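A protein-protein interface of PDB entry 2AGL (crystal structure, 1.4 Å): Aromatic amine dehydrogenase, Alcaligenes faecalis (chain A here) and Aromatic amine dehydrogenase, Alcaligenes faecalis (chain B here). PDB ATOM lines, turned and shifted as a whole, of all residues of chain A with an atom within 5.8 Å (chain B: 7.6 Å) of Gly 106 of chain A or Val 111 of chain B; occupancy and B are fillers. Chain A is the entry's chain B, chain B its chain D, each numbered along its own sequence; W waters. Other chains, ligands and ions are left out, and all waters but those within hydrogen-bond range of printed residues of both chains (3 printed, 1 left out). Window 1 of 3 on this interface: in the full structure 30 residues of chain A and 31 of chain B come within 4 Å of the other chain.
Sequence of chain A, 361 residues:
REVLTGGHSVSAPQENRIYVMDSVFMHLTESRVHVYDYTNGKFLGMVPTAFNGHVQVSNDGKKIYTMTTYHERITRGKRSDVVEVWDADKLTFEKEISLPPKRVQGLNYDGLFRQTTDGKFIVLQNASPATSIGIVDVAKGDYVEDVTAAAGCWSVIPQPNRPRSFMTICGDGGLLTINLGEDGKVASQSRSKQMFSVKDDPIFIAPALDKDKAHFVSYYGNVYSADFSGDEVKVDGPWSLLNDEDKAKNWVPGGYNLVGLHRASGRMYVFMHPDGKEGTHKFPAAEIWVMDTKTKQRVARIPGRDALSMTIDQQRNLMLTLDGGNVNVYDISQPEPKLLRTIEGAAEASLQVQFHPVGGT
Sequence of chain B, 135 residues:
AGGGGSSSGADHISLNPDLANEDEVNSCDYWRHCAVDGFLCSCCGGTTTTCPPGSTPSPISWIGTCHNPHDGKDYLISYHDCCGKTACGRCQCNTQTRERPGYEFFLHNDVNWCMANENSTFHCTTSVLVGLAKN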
ATOM      1  N   ASN A  52      37.661   7.763  -5.605  1.00  0.00           N
ATOM      2  CA  ASN A  52      36.503   8.004  -6.459  1.00  0.00           C
ATOM      3  C   ASN A  52      36.534   9.386  -7.090  1.00  0.00           C
ATOM      4  O   ASN A  52      35.613  10.180  -6.938  1.00  0.00           O
ATOM      5  CB  ASN A  52      35.230   7.810  -5.665  1.00  0.00           C
ATOM      6  CG  ASN A  52      33.974   7.997  -6.492  1.00  0.00           C
ATOM      7  OD1 ASN A  52      33.843   7.553  -7.673  1.00  0.00           O
ATOM      8  ND2 ASN A  52      33.017   8.644  -5.894  1.00  0.00           N
ATOM      9  N   GLY A  53      37.594   9.700  -7.830  1.00  0.00           N
ATOM     10  CA  GLY A  53      37.661  10.983  -8.514  1.00  0.00           C
ATOM     11  C   GLY A  53      36.639  11.161  -9.611  1.00  0.00           C
ATOM     12  O   GLY A  53      36.161  10.175 -10.201  1.00  0.00           O
ATOM     13  N   HIS A  54      36.273  12.430  -9.820  1.00  0.00           N
ATOM     14  CA  HIS A  54      35.500  12.858 -10.984  1.00  0.00           C
ATOM     15  C   HIS A  54      36.351  13.877 -11.724  1.00  0.00           C
ATOM     16  O   HIS A  54      37.256  14.509 -11.155  1.00  0.00           O
ATOM     17  CB  HIS A  54      34.153  13.464 -10.559  1.00  0.00           C
ATOM     18  CG  HIS A  54      33.186  12.458 -10.033  1.00  0.00           C
ATOM     19  ND1 HIS A  54      31.946  12.264 -10.588  1.00  0.00           N
ATOM     20  CD2 HIS A  54      33.301  11.541  -9.040  1.00  0.00           C
ATOM     21  CE1 HIS A  54      31.332  11.280  -9.963  1.00  0.00           C
ATOM     22  NE2 HIS A  54      32.127  10.832  -9.006  1.00  0.00           N
ATOM     23  N   ARG A 103      30.459  16.082  -1.088  1.00  0.00           N
ATOM     24  CA  ARG A 103      30.440  15.938  -2.549  1.00  0.00           C
ATOM     25  C   ARG A 103      29.996  14.518  -2.891  1.00  0.00           C
ATOM     26  O   ARG A 103      30.313  13.565  -2.194  1.00  0.00           O
ATOM     27  CB  ARG A 103      31.779  16.295  -3.198  1.00  0.00           C
ATOM     28  CG  ARG A 103      32.892  15.308  -2.934  1.00  0.00           C
ATOM     29  CD  ARG A 103      32.970  14.172  -3.937  1.00  0.00           C
ATOM     30  NE  ARG A 103      34.074  13.277  -3.652  1.00  0.00           N
ATOM     31  CZ  ARG A 103      34.393  12.229  -4.387  1.00  0.00           C
ATOM     32  NH1 ARG A 103      33.658  11.899  -5.439  1.00  0.00           N
ATOM     33  NH2 ARG A 103      35.463  11.513  -4.083  1.00  0.00           N
ATOM     34  N   VAL A 104      29.274  14.364  -4.001  1.00  0.00           N
ATOM     35  CA  VAL A 104      28.765  13.040  -4.345  1.00  0.00           C
ATOM     36  C   VAL A 104      29.889  12.046  -4.543  1.00  0.00           C
ATOM     37  O   VAL A 104      30.819  12.301  -5.323  1.00  0.00           O
ATOM     38  CB  VAL A 104      27.894  13.053  -5.631  1.00  0.00           C
ATOM     39  CG1 VAL A 104      28.643  13.569  -6.859  1.00  0.00           C
ATOM     40  CG2 VAL A 104      27.311  11.643  -5.882  1.00  0.00           C
ATOM     41  N   GLN A 105      29.784  10.910  -3.872  1.00  0.00           N
ATOM     42  CA  GLN A 105      30.649   9.750  -4.082  1.00  0.00           C
ATOM     43  C   GLN A 105      29.813   8.729  -4.820  1.00  0.00           C
ATOM     44  O   GLN A 105      28.803   8.243  -4.321  1.00  0.00           O
ATOM     45  CB  GLN A 105      31.176   9.234  -2.745  1.00  0.00           C
ATOM     46  CG  GLN A 105      32.176  10.223  -2.088  1.00  0.00           C
ATOM     47  CD  GLN A 105      32.648   9.810  -0.714  1.00  0.00           C
ATOM     48  OE1 GLN A 105      33.576  10.407  -0.138  1.00  0.00           O
ATOM     49  NE2 GLN A 105      32.008   8.815  -0.169  1.00  0.00           N
ATOM     50  N   GLY A 106      30.221   8.419  -6.045  1.00  0.00           N
ATOM     51  CA  GLY A 106      29.456   7.523  -6.880  1.00  0.00           C
ATOM     52  C   GLY A 106      30.058   7.426  -8.250  1.00  0.00           C
ATOM     53  O   GLY A 106      31.071   8.046  -8.583  1.00  0.00           O
ATOM     54  N   LEU A 107      29.403   6.616  -9.070  1.00  0.00           N
ATOM     55  CA  LEU A 107      29.899   6.344 -10.415  1.00  0.00           C
ATOM     56  C   LEU A 107      29.882   7.595 -11.261  1.00  0.00           C
ATOM     57  O   LEU A 107      29.148   8.547 -11.004  1.00  0.00           O
ATOM     58  CB  LEU A 107      29.076   5.236 -11.081  1.00  0.00           C
ATOM     59  CG  LEU A 107      28.997   3.933 -10.258  1.00  0.00           C
ATOM     60  CD1 LEU A 107      28.312   2.861 -11.037  1.00  0.00           C
ATOM     61  CD2 LEU A 107      30.344   3.416  -9.734  1.00  0.00           C
ATOM     62  N   ASN A 108      30.744   7.610 -12.297  1.00  0.00           N
ATOM     63  CA  ASN A 108      31.086   8.817 -13.053  1.00  0.00           C
ATOM     64  C   ASN A 108      30.103   9.196 -14.169  1.00  0.00           C
ATOM     65  O   ASN A 108      30.492   9.275 -15.327  1.00  0.00           O
ATOM     66  CB  ASN A 108      32.526   8.759 -13.598  1.00  0.00           C
ATOM     67  CG  ASN A 108      33.559   8.739 -12.476  1.00  0.00           C
ATOM     68  OD1 ASN A 108      33.931   9.803 -11.930  1.00  0.00           O
ATOM     69  ND2 ASN A 108      33.998   7.559 -12.117  1.00  0.00           N
ATOM     70  N   LEU A 112      27.190  14.713 -12.685  1.00  0.00           N
ATOM     71  CA  LEU A 112      27.556  14.908 -11.287  1.00  0.00           C
ATOM     72  C   LEU A 112      28.611  16.008 -11.086  1.00  0.00           C
ATOM     73  O   LEU A 112      28.830  16.479  -9.957  1.00  0.00           O
ATOM     74  CB  LEU A 112      27.994  13.567 -10.683  1.00  0.00           C
ATOM     75  CG  LEU A 112      26.894  12.521 -10.696  1.00  0.00           C
ATOM     76  CD1 LEU A 112      27.409  11.202 -10.104  1.00  0.00           C
ATOM     77  CD2 LEU A 112      25.600  12.928  -9.988  1.00  0.00           C
ATOM     78  N   TRP A 154      18.376  15.385  -8.728  1.00  0.00           N
ATOM     79  CA  TRP A 154      19.662  14.740  -9.013  1.00  0.00           C
ATOM     80  C   TRP A 154      20.200  15.125 -10.371  1.00  0.00           C
ATOM     81  O   TRP A 154      19.470  15.086 -11.378  1.00  0.00           O
ATOM     82  CB  TRP A 154      19.487  13.242  -8.964  1.00  0.00           C
ATOM     83  CG  TRP A 154      20.736  12.477  -8.841  1.00  0.00           C
ATOM     84  CD1 TRP A 154      21.276  11.602  -9.756  1.00  0.00           C
ATOM     85  CD2 TRP A 154      21.622  12.485  -7.720  1.00  0.00           C
ATOM     86  NE1 TRP A 154      22.427  11.056  -9.248  1.00  0.00           N
ATOM     87  CE2 TRP A 154      22.677  11.593  -8.009  1.00  0.00           C
ATOM     88  CE3 TRP A 154      21.635  13.165  -6.501  1.00  0.00           C
ATOM     89  CZ2 TRP A 154      23.717  11.361  -7.128  1.00  0.00           C
ATOM     90  CZ3 TRP A 154      22.658  12.934  -5.629  1.00  0.00           C
ATOM     91  CH2 TRP A 154      23.696  12.043  -5.941  1.00  0.00           C
ATOM     92  N   ASP B  37      25.271  -3.433  -5.722  1.00  0.00           N
ATOM     93  CA  ASP B  37      26.365  -2.906  -6.562  1.00  0.00           C
ATOM     94  C   ASP B  37      27.522  -2.775  -5.601  1.00  0.00           C
ATOM     95  O   ASP B  37      27.623  -1.787  -4.872  1.00  0.00           O
ATOM     96  CB  ASP B  37      25.991  -1.546  -7.178  1.00  0.00           C
ATOM     97  CG  ASP B  37      27.136  -0.854  -7.898  1.00  0.00           C
ATOM     98  OD1 ASP B  37      28.131  -1.509  -8.282  1.00  0.00           O
ATOM     99  OD2 ASP B  37      27.123   0.379  -8.148  1.00  0.00           O
ATOM    100  N   SER B  61      21.292   3.596   3.718  1.00  0.00           N
ATOM    101  CA  SER B  61      21.409   2.537   2.726  1.00  0.00           C
ATOM    102  C   SER B  61      20.464   2.773   1.597  1.00  0.00           C
ATOM    103  O   SER B  61      19.462   3.462   1.740  1.00  0.00           O
ATOM    104  CB  SER B  61      21.019   1.205   3.327  1.00  0.00           C
ATOM    105  OG  SER B  61      19.634   1.192   3.691  1.00  0.00           O
ATOM    106  N   TRQ B  62      20.748   2.136   0.479  1.00  0.00           N
ATOM    107  CA  TRQ B  62      19.709   1.920  -0.507  1.00  0.00           C
ATOM    108  C   TRQ B  62      18.943   0.657  -0.156  1.00  0.00           C
ATOM    109  O   TRQ B  62      19.413  -0.187   0.589  1.00  0.00           O
ATOM    110  CB  TRQ B  62      20.269   1.898  -1.925  1.00  0.00           C
ATOM    111  CG  TRQ B  62      21.262   0.818  -2.293  1.00  0.00           C
ATOM    112  CD1 TRQ B  62      20.933  -0.380  -2.815  1.00  0.00           C
ATOM    113  NE1 TRQ B  62      22.049  -1.105  -3.113  1.00  0.00           N
ATOM    114  CE2 TRQ B  62      23.169  -0.385  -2.802  1.00  0.00           C
ATOM    115  CZ2 TRQ B  62      24.512  -0.737  -2.957  1.00  0.00           C
ATOM    116  CH2 TRQ B  62      25.458   0.168  -2.576  1.00  0.00           C
ATOM    117  CZ3 TRQ B  62      25.082   1.427  -2.052  1.00  0.00           C
ATOM    118  CE3 TRQ B  62      23.718   1.781  -1.894  1.00  0.00           C
ATOM    119  CD2 TRQ B  62      22.736   0.849  -2.296  1.00  0.00           C
ATOM    120  O7  TRQ B  62      24.844  -1.873  -3.426  1.00  0.00           O
ATOM    121  N   ASP B  81      26.161  -0.557   3.649  1.00  0.00           N
ATOM    122  CA  ASP B  81      27.575  -0.792   3.348  1.00  0.00           C
ATOM    123  C   ASP B  81      28.345  -0.931   4.649  1.00  0.00           C
ATOM    124  O   ASP B  81      27.860  -0.596   5.739  1.00  0.00           O
ATOM    125  CB  ASP B  81      28.175   0.336   2.497  1.00  0.00           C
ATOM    126  CG  ASP B  81      27.691   0.344   1.070  1.00  0.00           C
ATOM    127  OD1 ASP B  81      27.250  -0.710   0.553  1.00  0.00           O
ATOM    128  OD2 ASP B  81      27.813   1.368   0.373  1.00  0.00           O
ATOM    129  N   GLU B  99      16.039  -1.213  -9.198  1.00  0.00           N
ATOM    130  CA  GLU B  99      16.915  -0.085  -8.911  1.00  0.00           C
ATOM    131  C   GLU B  99      16.547   1.085  -9.799  1.00  0.00           C
ATOM    132  O   GLU B  99      16.182   0.930 -10.973  1.00  0.00           O
ATOM    133  CB  GLU B  99      18.390  -0.480  -9.155  1.00  0.00           C
ATOM    134  CG  GLU B  99      19.424   0.532  -8.642  1.00  0.00           C
ATOM    135  CD  GLU B  99      19.799   1.631  -9.617  1.00  0.00           C
ATOM    136  OE1 GLU B  99      19.349   1.648 -10.797  1.00  0.00           O
ATOM    137  OE2 GLU B  99      20.603   2.515  -9.253  1.00  0.00           O
ATOM    138  N   GLY B 102      19.177   8.508  -9.290  1.00  0.00           N
ATOM    139  CA  GLY B 102      19.371   9.288  -8.063  1.00  0.00           C
ATOM    140  C   GLY B 102      18.221  10.223  -7.719  1.00  0.00           C
ATOM    141  O   GLY B 102      18.172  10.701  -6.591  1.00  0.00           O
ATOM    142  N   PHE B 105      16.319   8.536  -4.638  1.00  0.00           N
ATOM    143  CA  PHE B 105      17.686   8.350  -4.113  1.00  0.00           C
ATOM    144  C   PHE B 105      17.870   7.076  -3.327  1.00  0.00           C
ATOM    145  O   PHE B 105      18.914   6.414  -3.453  1.00  0.00           O
ATOM    146  CB  PHE B 105      18.154   9.568  -3.282  1.00  0.00           C
ATOM    147  CG  PHE B 105      19.668   9.700  -3.173  1.00  0.00           C
ATOM    148  CD1 PHE B 105      20.451   9.752  -4.305  1.00  0.00           C
ATOM    149  CD2 PHE B 105      20.299   9.802  -1.951  1.00  0.00           C
ATOM    150  CE1 PHE B 105      21.843   9.865  -4.223  1.00  0.00           C
ATOM    151  CE2 PHE B 105      21.671   9.933  -1.862  1.00  0.00           C
ATOM    152  CZ  PHE B 105      22.442   9.977  -2.999  1.00  0.00           C
ATOM    153  N   PHE B 106      16.895   6.696  -2.509  1.00  0.00           N
ATOM    154  CA  PHE B 106      17.075   5.514  -1.687  1.00  0.00           C
ATOM    155  C   PHE B 106      16.790   4.179  -2.383  1.00  0.00           C
ATOM    156  O   PHE B 106      16.883   3.129  -1.755  1.00  0.00           O
ATOM    157  CB  PHE B 106      16.337   5.689  -0.355  1.00  0.00           C
ATOM    158  CG  PHE B 106      16.889   6.817   0.465  1.00  0.00           C
ATOM    159  CD1 PHE B 106      16.311   8.084   0.403  1.00  0.00           C
ATOM    160  CD2 PHE B 106      18.011   6.633   1.235  1.00  0.00           C
ATOM    161  CE1 PHE B 106      16.849   9.140   1.129  1.00  0.00           C
ATOM    162  CE2 PHE B 106      18.555   7.689   1.982  1.00  0.00           C
ATOM    163  CZ  PHE B 106      17.973   8.933   1.926  1.00  0.00           C
ATOM    164  N   LEU B 107      16.487   4.236  -3.676  1.00  0.00           N
ATOM    165  CA  LEU B 107      16.415   3.046  -4.520  1.00  0.00           C
ATOM    166  C   LEU B 107      17.642   2.943  -5.420  1.00  0.00           C
ATOM    167  O   LEU B 107      17.688   2.071  -6.267  1.00  0.00           O
ATOM    168  CB  LEU B 107      15.161   3.111  -5.414  1.00  0.00           C
ATOM    169  CG  LEU B 107      13.819   3.073  -4.701  1.00  0.00           C
ATOM    170  CD1 LEU B 107      12.690   3.140  -5.745  1.00  0.00           C
ATOM    171  CD2 LEU B 107      13.660   1.853  -3.874  1.00  0.00           C
ATOM    172  N   HIS B 108      18.625   3.831  -5.245  1.00  0.00           N
ATOM    173  CA  HIS B 108      19.701   4.019  -6.196  1.00  0.00           C
ATOM    174  C   HIS B 108      21.007   3.398  -5.688  1.00  0.00           C
ATOM    175  O   HIS B 108      21.442   3.672  -4.555  1.00  0.00           O
ATOM    176  CB  HIS B 108      19.928   5.517  -6.396  1.00  0.00           C
ATOM    177  CG  HIS B 108      20.921   5.817  -7.467  1.00  0.00           C
ATOM    178  ND1 HIS B 108      21.910   6.770  -7.358  1.00  0.00           N
ATOM    179  CD2 HIS B 108      21.063   5.266  -8.689  1.00  0.00           C
ATOM    180  CE1 HIS B 108      22.626   6.784  -8.471  1.00  0.00           C
ATOM    181  NE2 HIS B 108      22.121   5.889  -9.297  1.00  0.00           N
ATOM    182  N   ASN B 109      21.681   2.600  -6.513  1.00  0.00           N
ATOM    183  CA  ASN B 109      22.896   1.903  -6.056  1.00  0.00           C
ATOM    184  C   ASN B 109      24.196   2.297  -6.790  1.00  0.00           C
ATOM    185  O   ASN B 109      25.175   1.582  -6.624  1.00  0.00           O
ATOM    186  CB  ASN B 109      22.702   0.386  -6.016  1.00  0.00           C
ATOM    187  CG  ASN B 109      22.689  -0.272  -7.372  1.00  0.00           C
ATOM    188  OD1 ASN B 109      22.984   0.348  -8.386  1.00  0.00           O
ATOM    189  ND2 ASN B 109      22.339  -1.567  -7.380  1.00  0.00           N
ATOM    190  N   ASP B 110      24.206   3.416  -7.509  1.00  0.00           N
ATOM    191  CA  ASP B 110      25.459   3.919  -8.119  1.00  0.00           C
ATOM    192  C   ASP B 110      26.110   5.027  -7.283  1.00  0.00           C
ATOM    193  O   ASP B 110      26.946   5.777  -7.770  1.00  0.00           O
ATOM    194  CB  ASP B 110      25.238   4.460  -9.528  1.00  0.00           C
ATOM    195  CG  ASP B 110      24.699   3.451 -10.502  1.00  0.00           C
ATOM    196  OD1 ASP B 110      24.875   2.243 -10.322  1.00  0.00           O
ATOM    197  OD2 ASP B 110      24.104   3.861 -11.522  1.00  0.00           O
ATOM    198  N   VAL B 111      25.689   5.121  -6.036  1.00  0.00           N
ATOM    199  CA  VAL B 111      26.334   5.993  -5.047  1.00  0.00           C
ATOM    200  C   VAL B 111      26.904   5.179  -3.889  1.00  0.00           C
ATOM    201  O   VAL B 111      26.472   4.077  -3.607  1.00  0.00           O
ATOM    202  CB  VAL B 111      25.397   7.097  -4.519  1.00  0.00           C
ATOM    203  CG1 VAL B 111      25.114   8.108  -5.628  1.00  0.00           C
ATOM    204  CG2 VAL B 111      24.104   6.506  -3.889  1.00  0.00           C
ATOM    205  N   ASN B 112      27.899   5.749  -3.222  1.00  0.00           N
ATOM    206  CA  ASN B 112      28.549   5.094  -2.098  1.00  0.00           C
ATOM    207  C   ASN B 112      27.692   5.274  -0.843  1.00  0.00           C
ATOM    208  O   ASN B 112      27.622   6.391  -0.341  1.00  0.00           O
ATOM    209  CB  ASN B 112      29.910   5.746  -1.898  1.00  0.00           C
ATOM    210  CG  ASN B 112      30.669   5.174  -0.738  1.00  0.00           C
ATOM    211  OD1 ASN B 112      30.396   4.069  -0.260  1.00  0.00           O
ATOM    212  ND2 ASN B 112      31.654   5.950  -0.268  1.00  0.00           N
ATOM    213  N   TRP B 113      27.033   4.227  -0.354  1.00  0.00           N
ATOM    214  CA  TRP B 113      26.171   4.362   0.819  1.00  0.00           C
ATOM    215  C   TRP B 113      26.975   4.543   2.116  1.00  0.00           C
ATOM    216  O   TRP B 113      26.376   4.726   3.176  1.00  0.00           O
ATOM    217  CB  TRP B 113      25.056   3.291   0.851  1.00  0.00           C
ATOM    218  CG  TRP B 113      23.949   3.749  -0.058  1.00  0.00           C
ATOM    219  CD1 TRP B 113      23.561   3.207  -1.277  1.00  0.00           C
ATOM    220  CD2 TRP B 113      23.136   4.903   0.125  1.00  0.00           C
ATOM    221  NE1 TRP B 113      22.550   3.949  -1.828  1.00  0.00           N
ATOM    222  CE2 TRP B 113      22.272   5.009  -0.993  1.00  0.00           C
ATOM    223  CE3 TRP B 113      23.005   5.836   1.163  1.00  0.00           C
ATOM    224  CZ2 TRP B 113      21.335   6.029  -1.113  1.00  0.00           C
ATOM    225  CZ3 TRP B 113      22.079   6.834   1.050  1.00  0.00           C
ATOM    226  CH2 TRP B 113      21.241   6.921  -0.075  1.00  0.00           C
ATOM    227  N   CYS B 114      28.318   4.540   2.018  1.00  0.00           N
ATOM    228  CA  CYS B 114      29.210   4.980   3.103  1.00  0.00           C
ATOM    229  C   CYS B 114      29.397   6.510   3.151  1.00  0.00           C
ATOM    230  O   CYS B 114      30.178   6.995   3.974  1.00  0.00           O
ATOM    231  CB  CYS B 114      30.606   4.360   2.924  1.00  0.00           C
ATOM    232  SG  CYS B 114      30.728   2.598   3.194  1.00  0.00           S
ATOM    233  N   MET B 115      28.704   7.250   2.279  1.00  0.00           N
ATOM    234  CA  MET B 115      28.974   8.682   2.081  1.00  0.00           C
ATOM    235  C   MET B 115      28.882   9.536   3.325  1.00  0.00           C
ATOM    236  O   MET B 115      29.456  10.618   3.333  1.00  0.00           O
ATOM    237  CB  MET B 115      28.038   9.282   1.034  1.00  0.00           C
ATOM    238  CG  MET B 115      26.579   9.284   1.482  1.00  0.00           C
ATOM    239  SD  MET B 115      25.443   9.851   0.170  1.00  0.00           S
ATOM    240  CE  MET B 115      25.080   8.345  -0.721  1.00  0.00           C
ATOM    241  N   PHE B 122      34.818   2.771   0.950  1.00  0.00           N
ATOM    242  CA  PHE B 122      33.894   1.664   0.765  1.00  0.00           C
ATOM    243  C   PHE B 122      34.593   0.320   0.838  1.00  0.00           C
ATOM    244  O   PHE B 122      35.549   0.062   0.106  1.00  0.00           O
ATOM    245  CB  PHE B 122      33.169   1.781  -0.563  1.00  0.00           C
ATOM    246  CG  PHE B 122      32.368   0.547  -0.915  1.00  0.00           C
ATOM    247  CD1 PHE B 122      31.207   0.193  -0.213  1.00  0.00           C
ATOM    248  CD2 PHE B 122      32.792  -0.284  -1.940  1.00  0.00           C
ATOM    249  CE1 PHE B 122      30.504  -0.917  -0.568  1.00  0.00           C
ATOM    250  CE2 PHE B 122      32.085  -1.410  -2.281  1.00  0.00           C
ATOM    251  CZ  PHE B 122      30.948  -1.722  -1.597  1.00  0.00           C
HETATM  252  O   HOH W   1      26.666   8.040  -9.469  1.00  0.00           O
HETATM  253  O   HOH W   2      27.183  10.202  -2.630  1.00  0.00           O
HETATM  254  O   HOH W   3      21.383   8.470 -11.303  1.00  0.00           O
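The backbone carbonyl oxygen of Asp 110 of chain B lies within hydrogen-bond range of the backbone NH of Leu 107 of chain A (2.9 Å). The backbone carbonyl oxygen (O) of Gln 105 of chain A sits at hydrogen-bond distance from the backbone NH (N) of Asn 112 of chain B, at 2.9 Å.
O7 of TRQ 62 of chain B sits at hydrogen-bond distance from N of Asp 37 of chain B (2.8 Å). The side-chain amide oxygen of Asn 109 of chain B lies close to the side-chain carboxylate of Asp 110 of chain B, 3.3 Å away. The backbone NH (N) of Cys 114 of chain B sits close to the side-chain amide oxygen (OD1) of Asn 112 of chain B (3.1 Å). N of Gly 106 of chain A lies close to ND2 of Asn 52 of chain A (2.8 Å). A ring nitrogen (NE2) of His 54 of chain A is in hydrogen-bond range of the backbone carbonyl oxygen of Gly 106 of chain A, at 3.0 Å.
Among the printed residues, pairs that only touch across the chains: Gln 105 of chain A with Val 111 of chain B (3.4 Å), Gln 105 of chain A with Met 115 of chain B (3.8 Å), Gly 106 of chain A with Asp 110 of chain B (3.2 Å), Gly 106 of chain A with Val 111 of chain B (3.9 Å), Leu 107 of chain A with Asp 37 of chain B (3.99 Å), Trp 154 of chain A with Gly 102 of chain B (3.4 Å), Trp 154 of chain A with Phe 105 of chain B (3.3 Å) and Trp 154 of chain A with Val 111 of chain B (3.8 Å).
Of chain B, only Asp 110 (3.2 Å) and Val 111 (3.9 Å) come within 4 Å of Gly 106 of chain A. Of the printed residues of chain A, Met 115 of chain B touches Gln 105 (3.8 Å). Printed residues of chain A within 4 Å of Gly 102 of chain B: Trp 154 (3.4 Å). Printed residues of chain B within 4 Å of Leu 107 of chain A: Asp 37 (3.99 Å) and Asp 110 (2.9 Å). Printed residues of chain A within 4 Å of Phe 105 of chain B: Trp 154. Printed residues of chain A within 4 Å of Asp 110 of chain B: Gly 106 (3.2 Å) and Leu 107 (2.9 Å). TRQ 62 of chain B touches none of the printed residues of chain A. Asn 108 of chain A touches none of the printed residues of chain B. The nearest residue of chain A that does not touch Val 111 of chain B is Val 104 of chain A (4.2 Å). The nearest printed residue of chain A that does not touch Asp 37 of chain B is Gly 106 of chain A (7.6 Å).
Of the 11 printed residues of chain A, 4 touch a printed residue of chain B. Of the 18 printed residues of chain B, 7 touch a printed residue of chain A. Along chain B the printed residues that touch a printed residue of chain A span positions 37 to 115. Among the printed residues, 10 pairs touch across the chains.
Water W1 bridges O of Asp 110 of chain B and O of Leu 107 of chain A. Water W2 lies within hydrogen-bond range of the backbone NH (N) of Gln 105 of chain A (3.0 Å) and the side-chain sulfur (SD) of Met 115 of chain B (3.3 Å). Water W3 lies within hydrogen-bond range of the backbone NH of Gly 102 of chain B (3.0 Å), a ring nitrogen (NE2) of His 108 of chain B (3.4 Å) and the indole nitrogen of Trp 154 of chain A (3.5 Å).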
